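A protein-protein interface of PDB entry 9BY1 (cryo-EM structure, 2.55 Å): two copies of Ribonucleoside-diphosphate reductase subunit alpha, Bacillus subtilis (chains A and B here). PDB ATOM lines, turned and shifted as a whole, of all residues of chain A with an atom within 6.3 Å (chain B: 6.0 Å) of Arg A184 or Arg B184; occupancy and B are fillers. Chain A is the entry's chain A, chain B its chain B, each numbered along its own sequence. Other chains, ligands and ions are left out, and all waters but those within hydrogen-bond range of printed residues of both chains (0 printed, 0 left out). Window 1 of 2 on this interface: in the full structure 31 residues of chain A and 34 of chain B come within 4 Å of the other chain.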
ATOM      1  N   LEU A 173     -15.028  -5.379  17.506  1.00  0.00           N
ATOM      2  CA  LEU A 173     -14.360  -4.245  18.126  1.00  0.00           C
ATOM      3  C   LEU A 173     -15.148  -2.968  17.884  1.00  0.00           C
ATOM      4  O   LEU A 173     -15.611  -2.713  16.769  1.00  0.00           O
ATOM      5  CB  LEU A 173     -12.938  -4.067  17.586  1.00  0.00           C
ATOM      6  CG  LEU A 173     -11.987  -5.262  17.591  1.00  0.00           C
ATOM      7  CD1 LEU A 173     -10.621  -4.823  17.098  1.00  0.00           C
ATOM      8  CD2 LEU A 173     -11.892  -5.887  18.970  1.00  0.00           C
ATOM      9  N   LEU A 179      -7.797   9.368  17.212  1.00  0.00           N
ATOM     10  CA  LEU A 179      -6.636   8.758  16.570  1.00  0.00           C
ATOM     11  C   LEU A 179      -6.001   7.704  17.465  1.00  0.00           C
ATOM     12  O   LEU A 179      -5.498   6.688  16.974  1.00  0.00           O
ATOM     13  CB  LEU A 179      -5.613   9.830  16.199  1.00  0.00           C
ATOM     14  CG  LEU A 179      -4.440   9.369  15.331  1.00  0.00           C
ATOM     15  CD1 LEU A 179      -4.908   9.052  13.920  1.00  0.00           C
ATOM     16  CD2 LEU A 179      -3.339  10.414  15.318  1.00  0.00           C
ATOM     17  N   ASN A 180      -6.000   7.935  18.780  1.00  0.00           N
ATOM     18  CA  ASN A 180      -5.512   6.918  19.706  1.00  0.00           C
ATOM     19  C   ASN A 180      -6.347   5.651  19.608  1.00  0.00           C
ATOM     20  O   ASN A 180      -5.806   4.538  19.572  1.00  0.00           O
ATOM     21  CB  ASN A 180      -5.532   7.458  21.136  1.00  0.00           C
ATOM     22  CG  ASN A 180      -4.323   8.310  21.455  1.00  0.00           C
ATOM     23  OD1 ASN A 180      -3.265   8.159  20.846  1.00  0.00           O
ATOM     24  ND2 ASN A 180      -4.474   9.210  22.418  1.00  0.00           N
ATOM     25  N   ASP A 181      -7.670   5.803  19.540  1.00  0.00           N
ATOM     26  CA  ASP A 181      -8.547   4.646  19.432  1.00  0.00           C
ATOM     27  C   ASP A 181      -8.428   3.971  18.073  1.00  0.00           C
ATOM     28  O   ASP A 181      -8.536   2.747  17.988  1.00  0.00           O
ATOM     29  CB  ASP A 181      -9.988   5.061  19.708  1.00  0.00           C
ATOM     30  CG  ASP A 181     -10.243   5.314  21.180  1.00  0.00           C
ATOM     31  OD1 ASP A 181     -10.388   4.331  21.935  1.00  0.00           O
ATOM     32  OD2 ASP A 181     -10.298   6.494  21.584  1.00  0.00           O
ATOM     33  N   ILE A 182      -8.191   4.737  17.007  1.00  0.00           N
ATOM     34  CA  ILE A 182      -8.002   4.130  15.692  1.00  0.00           C
ATOM     35  C   ILE A 182      -6.697   3.341  15.649  1.00  0.00           C
ATOM     36  O   ILE A 182      -6.642   2.231  15.103  1.00  0.00           O
ATOM     37  CB  ILE A 182      -8.058   5.212  14.598  1.00  0.00           C
ATOM     38  CG1 ILE A 182      -9.499   5.675  14.392  1.00  0.00           C
ATOM     39  CG2 ILE A 182      -7.475   4.694  13.292  1.00  0.00           C
ATOM     40  CD1 ILE A 182      -9.624   6.917  13.556  1.00  0.00           C
ATOM     41  N   SER A 183      -5.630   3.896  16.227  1.00  0.00           N
ATOM     42  CA  SER A 183      -4.365   3.173  16.302  1.00  0.00           C
ATOM     43  C   SER A 183      -4.505   1.905  17.133  1.00  0.00           C
ATOM     44  O   SER A 183      -3.991   0.845  16.757  1.00  0.00           O
ATOM     45  CB  SER A 183      -3.281   4.075  16.889  1.00  0.00           C
ATOM     46  OG  SER A 183      -3.255   5.333  16.242  1.00  0.00           O
ATOM     47  N   ARG A 184      -5.202   1.994  18.269  1.00  0.00           N
ATOM     48  CA  ARG A 184      -5.429   0.806  19.079  1.00  0.00           C
ATOM     49  C   ARG A 184      -6.291  -0.213  18.352  1.00  0.00           C
ATOM     50  O   ARG A 184      -6.077  -1.417  18.505  1.00  0.00           O
ATOM     51  CB  ARG A 184      -6.068   1.187  20.412  1.00  0.00           C
ATOM     52  CG  ARG A 184      -5.815   0.175  21.510  1.00  0.00           C
ATOM     53  CD  ARG A 184      -4.594   0.546  22.326  1.00  0.00           C
ATOM     54  NE  ARG A 184      -3.549  -0.465  22.231  1.00  0.00           N
ATOM     55  CZ  ARG A 184      -2.393  -0.406  22.878  1.00  0.00           C
ATOM     56  NH1 ARG A 184      -2.101   0.605  23.679  1.00  0.00           N
ATOM     57  NH2 ARG A 184      -1.509  -1.387  22.717  1.00  0.00           N
ATOM     58  N   ALA A 185      -7.267   0.241  17.565  1.00  0.00           N
ATOM     59  CA  ALA A 185      -8.079  -0.681  16.782  1.00  0.00           C
ATOM     60  C   ALA A 185      -7.237  -1.408  15.745  1.00  0.00           C
ATOM     61  O   ALA A 185      -7.390  -2.616  15.553  1.00  0.00           O
ATOM     62  CB  ALA A 185      -9.229   0.069  16.112  1.00  0.00           C
ATOM     63  N   ILE A 186      -6.338  -0.687  15.072  1.00  0.00           N
ATOM     64  CA  ILE A 186      -5.445  -1.327  14.107  1.00  0.00           C
ATOM     65  C   ILE A 186      -4.553  -2.347  14.803  1.00  0.00           C
ATOM     66  O   ILE A 186      -4.371  -3.475  14.321  1.00  0.00           O
ATOM     67  CB  ILE A 186      -4.613  -0.267  13.364  1.00  0.00           C
ATOM     68  CG1 ILE A 186      -5.493   0.550  12.421  1.00  0.00           C
ATOM     69  CG2 ILE A 186      -3.472  -0.917  12.596  1.00  0.00           C
ATOM     70  CD1 ILE A 186      -4.857   1.848  11.984  1.00  0.00           C
ATOM     71  N   ASP A 187      -3.988  -1.969  15.951  1.00  0.00           N
ATOM     72  CA  ASP A 187      -3.111  -2.872  16.688  1.00  0.00           C
ATOM     73  C   ASP A 187      -3.854  -4.126  17.130  1.00  0.00           C
ATOM     74  O   ASP A 187      -3.363  -5.245  16.957  1.00  0.00           O
ATOM     75  CB  ASP A 187      -2.513  -2.147  17.894  1.00  0.00           C
ATOM     76  CG  ASP A 187      -1.910  -3.096  18.910  1.00  0.00           C
ATOM     77  OD1 ASP A 187      -1.077  -3.940  18.519  1.00  0.00           O
ATOM     78  OD2 ASP A 187      -2.272  -3.002  20.101  1.00  0.00           O
ATOM     79  N   ILE A 188      -5.052  -3.955  17.693  1.00  0.00           N
ATOM     80  CA  ILE A 188      -5.824  -5.092  18.185  1.00  0.00           C
ATOM     81  C   ILE A 188      -6.284  -5.965  17.026  1.00  0.00           C
ATOM     82  O   ILE A 188      -6.319  -7.195  17.137  1.00  0.00           O
ATOM     83  CB  ILE A 188      -7.009  -4.599  19.036  1.00  0.00           C
ATOM     84  CG1 ILE A 188      -6.506  -3.971  20.335  1.00  0.00           C
ATOM     85  CG2 ILE A 188      -7.956  -5.737  19.357  1.00  0.00           C
ATOM     86  CD1 ILE A 188      -7.604  -3.406  21.198  1.00  0.00           C
ATOM     87  N   SER A 189      -6.638  -5.350  15.896  1.00  0.00           N
ATOM     88  CA  SER A 189      -7.021  -6.124  14.724  1.00  0.00           C
ATOM     89  C   SER A 189      -5.866  -6.984  14.236  1.00  0.00           C
ATOM     90  O   SER A 189      -6.055  -8.160  13.912  1.00  0.00           O
ATOM     91  CB  SER A 189      -7.498  -5.190  13.613  1.00  0.00           C
ATOM     92  OG  SER A 189      -8.478  -4.288  14.092  1.00  0.00           O
ATOM     93  N   TYR A 394      -9.324   4.562  24.597  1.00  0.00           N
ATOM     94  CA  TYR A 394      -7.875   4.434  24.642  1.00  0.00           C
ATOM     95  C   TYR A 394      -7.254   5.823  24.603  1.00  0.00           C
ATOM     96  O   TYR A 394      -7.418   6.558  23.623  1.00  0.00           O
ATOM     97  CB  TYR A 394      -7.376   3.573  23.485  1.00  0.00           C
ATOM     98  CG  TYR A 394      -7.878   2.148  23.537  1.00  0.00           C
ATOM     99  CD1 TYR A 394      -7.400   1.258  24.489  1.00  0.00           C
ATOM    100  CD2 TYR A 394      -8.833   1.694  22.638  1.00  0.00           C
ATOM    101  CE1 TYR A 394      -7.855  -0.042  24.541  1.00  0.00           C
ATOM    102  CE2 TYR A 394      -9.294   0.396  22.682  1.00  0.00           C
ATOM    103  CZ  TYR A 394      -8.803  -0.469  23.636  1.00  0.00           C
ATOM    104  OH  TYR A 394      -9.262  -1.765  23.684  1.00  0.00           O
ATOM    105  N   TYR A 397      -0.361   7.630  25.935  1.00  0.00           N
ATOM    106  CA  TYR A 397       0.486   6.592  26.513  1.00  0.00           C
ATOM    107  C   TYR A 397       0.585   6.729  28.026  1.00  0.00           C
ATOM    108  O   TYR A 397       0.525   5.731  28.753  1.00  0.00           O
ATOM    109  CB  TYR A 397       1.877   6.640  25.879  1.00  0.00           C
ATOM    110  CG  TYR A 397       2.809   5.560  26.374  1.00  0.00           C
ATOM    111  CD1 TYR A 397       2.820   4.304  25.785  1.00  0.00           C
ATOM    112  CD2 TYR A 397       3.673   5.794  27.435  1.00  0.00           C
ATOM    113  CE1 TYR A 397       3.667   3.312  26.236  1.00  0.00           C
ATOM    114  CE2 TYR A 397       4.521   4.809  27.894  1.00  0.00           C
ATOM    115  CZ  TYR A 397       4.516   3.572  27.290  1.00  0.00           C
ATOM    116  OH  TYR A 397       5.362   2.590  27.744  1.00  0.00           O
ATOM    117  N   ASP A 401      -6.357   3.864  30.278  1.00  0.00           N
ATOM    118  CA  ASP A 401      -7.391   3.646  29.278  1.00  0.00           C
ATOM    119  C   ASP A 401      -8.678   3.173  29.936  1.00  0.00           C
ATOM    120  O   ASP A 401      -8.652   2.390  30.889  1.00  0.00           O
ATOM    121  CB  ASP A 401      -6.935   2.619  28.243  1.00  0.00           C
ATOM    122  CG  ASP A 401      -5.646   3.014  27.556  1.00  0.00           C
ATOM    123  OD1 ASP A 401      -5.382   4.227  27.433  1.00  0.00           O
ATOM    124  OD2 ASP A 401      -4.895   2.110  27.136  1.00  0.00           O
ATOM    125  N   ASN A 447      -3.754  -9.160  24.513  1.00  0.00           N
ATOM    126  CA  ASN A 447      -3.460  -7.990  23.699  1.00  0.00           C
ATOM    127  C   ASN A 447      -4.711  -7.267  23.225  1.00  0.00           C
ATOM    128  O   ASN A 447      -4.595  -6.269  22.507  1.00  0.00           O
ATOM    129  CB  ASN A 447      -2.600  -8.380  22.489  1.00  0.00           C
ATOM    130  CG  ASN A 447      -1.191  -7.835  22.582  1.00  0.00           C
ATOM    131  OD1 ASN A 447      -0.988  -6.642  22.800  1.00  0.00           O
ATOM    132  ND2 ASN A 447      -0.208  -8.712  22.428  1.00  0.00           N
ATOM    133  N   PRO A 449      -7.641  -5.748  25.337  1.00  0.00           N
ATOM    134  CA  PRO A 449      -8.174  -5.590  26.701  1.00  0.00           C
ATOM    135  C   PRO A 449      -9.686  -5.672  26.782  1.00  0.00           C
ATOM    136  O   PRO A 449     -10.223  -6.257  27.731  1.00  0.00           O
ATOM    137  CB  PRO A 449      -7.663  -4.202  27.119  1.00  0.00           C
ATOM    138  CG  PRO A 449      -6.627  -3.832  26.110  1.00  0.00           C
ATOM    139  CD  PRO A 449      -6.978  -4.528  24.853  1.00  0.00           C
ATOM    140  N   LEU B 173      12.452   7.130  14.803  1.00  0.00           N
ATOM    141  CA  LEU B 173      11.940   6.028  15.600  1.00  0.00           C
ATOM    142  C   LEU B 173      12.666   4.736  15.256  1.00  0.00           C
ATOM    143  O   LEU B 173      12.888   4.430  14.082  1.00  0.00           O
ATOM    144  CB  LEU B 173      10.439   5.837  15.376  1.00  0.00           C
ATOM    145  CG  LEU B 173       9.535   7.063  15.470  1.00  0.00           C
ATOM    146  CD1 LEU B 173       8.088   6.631  15.325  1.00  0.00           C
ATOM    147  CD2 LEU B 173       9.750   7.799  16.780  1.00  0.00           C
ATOM    148  N   LEU B 179       5.323  -7.678  16.415  1.00  0.00           N
ATOM    149  CA  LEU B 179       4.060  -7.080  15.996  1.00  0.00           C
ATOM    150  C   LEU B 179       3.635  -5.968  16.946  1.00  0.00           C
ATOM    151  O   LEU B 179       3.086  -4.951  16.511  1.00  0.00           O
ATOM    152  CB  LEU B 179       2.972  -8.148  15.901  1.00  0.00           C
ATOM    153  CG  LEU B 179       1.638  -7.682  15.312  1.00  0.00           C
ATOM    154  CD1 LEU B 179       1.787  -7.359  13.834  1.00  0.00           C
ATOM    155  CD2 LEU B 179       0.558  -8.725  15.529  1.00  0.00           C
ATOM    156  N   ASN B 180       3.875  -6.148  18.246  1.00  0.00           N
ATOM    157  CA  ASN B 180       3.579  -5.096  19.213  1.00  0.00           C
ATOM    158  C   ASN B 180       4.361  -3.830  18.892  1.00  0.00           C
ATOM    159  O   ASN B 180       3.804  -2.726  18.864  1.00  0.00           O
ATOM    160  CB  ASN B 180       3.907  -5.581  20.625  1.00  0.00           C
ATOM    161  CG  ASN B 180       2.806  -6.424  21.227  1.00  0.00           C
ATOM    162  OD1 ASN B 180       1.659  -6.370  20.789  1.00  0.00           O
ATOM    163  ND2 ASN B 180       3.149  -7.213  22.237  1.00  0.00           N
ATOM    164  N   ASP B 181       5.658  -3.980  18.623  1.00  0.00           N
ATOM    165  CA  ASP B 181       6.497  -2.828  18.324  1.00  0.00           C
ATOM    166  C   ASP B 181       6.148  -2.208  16.977  1.00  0.00           C
ATOM    167  O   ASP B 181       6.214  -0.987  16.831  1.00  0.00           O
ATOM    168  CB  ASP B 181       7.967  -3.236  18.368  1.00  0.00           C
ATOM    169  CG  ASP B 181       8.431  -3.573  19.771  1.00  0.00           C
ATOM    170  OD1 ASP B 181       8.571  -2.644  20.592  1.00  0.00           O
ATOM    171  OD2 ASP B 181       8.657  -4.768  20.055  1.00  0.00           O
ATOM    172  N   ILE B 182       5.768  -3.021  15.991  1.00  0.00           N
ATOM    173  CA  ILE B 182       5.372  -2.478  14.694  1.00  0.00           C
ATOM    174  C   ILE B 182       4.075  -1.683  14.815  1.00  0.00           C
ATOM    175  O   ILE B 182       3.943  -0.591  14.244  1.00  0.00           O
ATOM    176  CB  ILE B 182       5.256  -3.613  13.660  1.00  0.00           C
ATOM    177  CG1 ILE B 182       6.648  -4.044  13.200  1.00  0.00           C
ATOM    178  CG2 ILE B 182       4.411  -3.183  12.473  1.00  0.00           C
ATOM    179  CD1 ILE B 182       6.668  -5.364  12.483  1.00  0.00           C
ATOM    180  N   SER B 183       3.101  -2.212  15.556  1.00  0.00           N
ATOM    181  CA  SER B 183       1.858  -1.479  15.776  1.00  0.00           C
ATOM    182  C   SER B 183       2.109  -0.187  16.540  1.00  0.00           C
ATOM    183  O   SER B 183       1.528   0.857  16.221  1.00  0.00           O
ATOM    184  CB  SER B 183       0.858  -2.358  16.522  1.00  0.00           C
ATOM    185  OG  SER B 183       1.422  -2.872  17.713  1.00  0.00           O
ATOM    186  N   ARG B 184       2.975  -0.236  17.556  1.00  0.00           N
ATOM    187  CA  ARG B 184       3.311   0.978  18.290  1.00  0.00           C
ATOM    188  C   ARG B 184       4.031   1.981  17.398  1.00  0.00           C
ATOM    189  O   ARG B 184       3.825   3.189  17.526  1.00  0.00           O
ATOM    190  CB  ARG B 184       4.163   0.637  19.511  1.00  0.00           C
ATOM    191  CG  ARG B 184       4.408   1.817  20.428  1.00  0.00           C
ATOM    192  CD  ARG B 184       3.123   2.552  20.746  1.00  0.00           C
ATOM    193  NE  ARG B 184       2.457   1.992  21.914  1.00  0.00           N
ATOM    194  CZ  ARG B 184       1.184   2.198  22.222  1.00  0.00           C
ATOM    195  NH1 ARG B 184       0.402   2.948  21.462  1.00  0.00           N
ATOM    196  NH2 ARG B 184       0.683   1.640  23.319  1.00  0.00           N
ATOM    197  N   ALA B 185       4.890   1.499  16.499  1.00  0.00           N
ATOM    198  CA  ALA B 185       5.565   2.389  15.563  1.00  0.00           C
ATOM    199  C   ALA B 185       4.569   3.067  14.636  1.00  0.00           C
ATOM    200  O   ALA B 185       4.685   4.265  14.363  1.00  0.00           O
ATOM    201  CB  ALA B 185       6.605   1.613  14.755  1.00  0.00           C
ATOM    202  N   ILE B 186       3.581   2.318  14.143  1.00  0.00           N
ATOM    203  CA  ILE B 186       2.547   2.916  13.300  1.00  0.00           C
ATOM    204  C   ILE B 186       1.766   3.966  14.083  1.00  0.00           C
ATOM    205  O   ILE B 186       1.500   5.069  13.585  1.00  0.00           O
ATOM    206  CB  ILE B 186       1.621   1.823  12.734  1.00  0.00           C
ATOM    207  CG1 ILE B 186       2.299   1.101  11.569  1.00  0.00           C
ATOM    208  CG2 ILE B 186       0.292   2.412  12.288  1.00  0.00           C
ATOM    209  CD1 ILE B 186       1.984  -0.371  11.507  1.00  0.00           C
ATOM    210  N   ASP B 187       1.403   3.644  15.326  1.00  0.00           N
ATOM    211  CA  ASP B 187       0.664   4.589  16.158  1.00  0.00           C
ATOM    212  C   ASP B 187       1.466   5.863  16.396  1.00  0.00           C
ATOM    213  O   ASP B 187       0.948   6.973  16.244  1.00  0.00           O
ATOM    214  CB  ASP B 187       0.296   3.930  17.486  1.00  0.00           C
ATOM    215  CG  ASP B 187      -0.038   4.940  18.566  1.00  0.00           C
ATOM    216  OD1 ASP B 187      -0.927   5.787  18.338  1.00  0.00           O
ATOM    217  OD2 ASP B 187       0.592   4.888  19.642  1.00  0.00           O
ATOM    218  N   ILE B 188       2.740   5.719  16.766  1.00  0.00           N
ATOM    219  CA  ILE B 188       3.570   6.880  17.066  1.00  0.00           C
ATOM    220  C   ILE B 188       3.831   7.693  15.806  1.00  0.00           C
ATOM    221  O   ILE B 188       3.879   8.926  15.849  1.00  0.00           O
ATOM    222  CB  ILE B 188       4.880   6.438  17.742  1.00  0.00           C
ATOM    223  CG1 ILE B 188       4.597   5.814  19.106  1.00  0.00           C
ATOM    224  CG2 ILE B 188       5.815   7.613  17.920  1.00  0.00           C
ATOM    225  CD1 ILE B 188       5.820   5.228  19.762  1.00  0.00           C
ATOM    226  N   SER B 189       4.005   7.021  14.667  1.00  0.00           N
ATOM    227  CA  SER B 189       4.175   7.735  13.408  1.00  0.00           C
ATOM    228  C   SER B 189       2.945   8.567  13.081  1.00  0.00           C
ATOM    229  O   SER B 189       3.065   9.723  12.669  1.00  0.00           O
ATOM    230  CB  SER B 189       4.470   6.746  12.282  1.00  0.00           C
ATOM    231  OG  SER B 189       5.605   5.958  12.587  1.00  0.00           O
ATOM    232  N   TYR B 394       8.204  -2.527  23.236  1.00  0.00           N
ATOM    233  CA  TYR B 394       6.788  -2.361  23.538  1.00  0.00           C
ATOM    234  C   TYR B 394       6.169  -3.741  23.703  1.00  0.00           C
ATOM    235  O   TYR B 394       6.060  -4.501  22.737  1.00  0.00           O
ATOM    236  CB  TYR B 394       6.094  -1.564  22.438  1.00  0.00           C
ATOM    237  CG  TYR B 394       6.619  -0.156  22.290  1.00  0.00           C
ATOM    238  CD1 TYR B 394       6.334   0.816  23.239  1.00  0.00           C
ATOM    239  CD2 TYR B 394       7.406   0.200  21.204  1.00  0.00           C
ATOM    240  CE1 TYR B 394       6.812   2.103  23.106  1.00  0.00           C
ATOM    241  CE2 TYR B 394       7.889   1.484  21.063  1.00  0.00           C
ATOM    242  CZ  TYR B 394       7.591   2.431  22.017  1.00  0.00           C
ATOM    243  OH  TYR B 394       8.072   3.713  21.878  1.00  0.00           O
ATOM    244  N   THR B 395       5.772  -4.064  24.926  1.00  0.00           N
ATOM    245  CA  THR B 395       5.276  -5.387  25.268  1.00  0.00           C
ATOM    246  C   THR B 395       3.758  -5.431  25.098  1.00  0.00           C
ATOM    247  O   THR B 395       3.149  -4.537  24.503  1.00  0.00           O
ATOM    248  CB  THR B 395       5.703  -5.746  26.688  1.00  0.00           C
ATOM    249  OG1 THR B 395       5.129  -4.810  27.607  1.00  0.00           O
ATOM    250  CG2 THR B 395       7.215  -5.698  26.811  1.00  0.00           C
ATOM    251  N   TYR B 397      -0.295  -5.383  26.231  1.00  0.00           N
ATOM    252  CA  TYR B 397      -1.026  -4.288  26.859  1.00  0.00           C
ATOM    253  C   TYR B 397      -0.913  -4.338  28.379  1.00  0.00           C
ATOM    254  O   TYR B 397      -0.755  -3.299  29.030  1.00  0.00           O
ATOM    255  CB  TYR B 397      -2.491  -4.324  26.422  1.00  0.00           C
ATOM    256  CG  TYR B 397      -3.362  -3.278  27.080  1.00  0.00           C
ATOM    257  CD1 TYR B 397      -3.986  -3.527  28.295  1.00  0.00           C
ATOM    258  CD2 TYR B 397      -3.560  -2.040  26.484  1.00  0.00           C
ATOM    259  CE1 TYR B 397      -4.778  -2.577  28.898  1.00  0.00           C
ATOM    260  CE2 TYR B 397      -4.353  -1.082  27.081  1.00  0.00           C
ATOM    261  CZ  TYR B 397      -4.960  -1.357  28.288  1.00  0.00           C
ATOM    262  OH  TYR B 397      -5.750  -0.407  28.888  1.00  0.00           O
ATOM    263  N   ASP B 401       6.149  -1.579  29.236  1.00  0.00           N
ATOM    264  CA  ASP B 401       7.037  -1.398  28.098  1.00  0.00           C
ATOM    265  C   ASP B 401       8.427  -0.973  28.555  1.00  0.00           C
ATOM    266  O   ASP B 401       8.595  -0.323  29.591  1.00  0.00           O
ATOM    267  CB  ASP B 401       6.473  -0.353  27.136  1.00  0.00           C
ATOM    268  CG  ASP B 401       5.144  -0.762  26.543  1.00  0.00           C
ATOM    269  OD1 ASP B 401       4.948  -1.968  26.291  1.00  0.00           O
ATOM    270  OD2 ASP B 401       4.294   0.125  26.328  1.00  0.00           O
ATOM    271  N   ASN B 447       2.536  11.071  23.266  1.00  0.00           N
ATOM    272  CA  ASN B 447       2.227   9.803  22.624  1.00  0.00           C
ATOM    273  C   ASN B 447       3.444   9.111  22.029  1.00  0.00           C
ATOM    274  O   ASN B 447       3.289   8.072  21.378  1.00  0.00           O
ATOM    275  CB  ASN B 447       1.167  10.005  21.536  1.00  0.00           C
ATOM    276  CG  ASN B 447      -0.241   9.845  22.065  1.00  0.00           C
ATOM    277  OD1 ASN B 447      -0.681   8.736  22.363  1.00  0.00           O
ATOM    278  ND2 ASN B 447      -0.954  10.956  22.191  1.00  0.00           N
ATOM    279  N   PRO B 449       6.673   7.857  23.835  1.00  0.00           N
ATOM    280  CA  PRO B 449       7.429   7.809  25.098  1.00  0.00           C
ATOM    281  C   PRO B 449       8.932   7.810  24.898  1.00  0.00           C
ATOM    282  O   PRO B 449       9.655   8.426  25.690  1.00  0.00           O
ATOM    283  CB  PRO B 449       6.940   6.511  25.760  1.00  0.00           C
ATOM    284  CG  PRO B 449       5.983   5.871  24.800  1.00  0.00           C
ATOM    285  CD  PRO B 449       6.068   6.562  23.491  1.00  0.00           C
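Of chain B, only Arg B184 comes within 4 Å of Arg A184. Arg B184 touches just one residue of chain A: Arg A184 (3.0 Å). Printed residues of chain B within 4 Å of Asn A180: Asn B447 (3.1 Å). Of the printed residues of chain A, Tyr B397 touches Asp A401 (3.2 Å), Asn A447 (3.7 Å) and Pro A449 (3.4 Å). Of the printed residues of chain A, Ser B183 touches Asp A187. Of the printed residues of chain B, Ser A183 touches Asp B187 (3.2 Å). Leu A173 touches none of the printed residues of chain B. Leu A179 touches none of the printed residues of chain B. The nearest residue of chain B that does not touch Arg A184 is Tyr B397 (4.1 Å). The nearest residue of chain A that does not touch Arg B184 is Tyr A397 (4.2 Å).
OD1 of Asn A180 sits close to OD1 of Asn B447. OG of Ser A183 lies within hydrogen-bond range of OD1 of Asp B187 (3.2 Å). The side-chain carboxylate (OD1) of Asp A187 sits at hydrogen-bond distance from the side-chain hydroxyl (OG) of Ser B183. OH of Tyr A397 is in hydrogen-bond range of OD2 of Asp B401 (3.0 Å). The side-chain carboxylate of Asp A401 sits at hydrogen-bond distance from the side-chain hydroxyl of Tyr B397, at 3.2 Å. OD1 of Asn B180 sits close to OD1 of Asn A447 (3.3 Å). The guanidinium group of Arg B184 sits close to the guanidinium group of Arg A184, 3.0 Å away.
Ser A183 touches Asp B187, and with the chains exchanged Asp A187 touches Ser B183. Arg B184 touches its own counterpart, Arg A184. Tyr A397 touches Asp B401, and with the chains exchanged Asp A401 touches Tyr B397. Tyr A397 touches Asn B447, and with the chains exchanged Asn A447 touches Tyr B397. 17 positions are printed for both chains.
O of Leu A179 sits at hydrogen-bond distance from OG of Ser A183 (2.7 Å). NH2 of Arg A184 is in salt-bridge range of OD2 of Asp A187 (3.2 Å). O of Leu B179 sits at hydrogen-bond distance from OG of Ser B183, 2.9 Å away. O of Asn B180 is in hydrogen-bond range of OG of Ser B183 (2.6 Å). The guanidinium group (NH1) of Arg B184 is in salt-bridge range of the side-chain carboxylate (OD2) of Asp B187 (2.7 Å). The side-chain carboxylate of Asp B401 lies within hydrogen-bond range of the backbone NH of Thr B395.
Of the 17 printed residues of chain A, 8 touch a printed residue of chain B.
Among the printed residues, merely in contact across the chains: Tyr A397 with Asn B447, Tyr A397 with Pro B449, Asn A447 with Tyr B397 and Pro A449 with Tyr B397.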
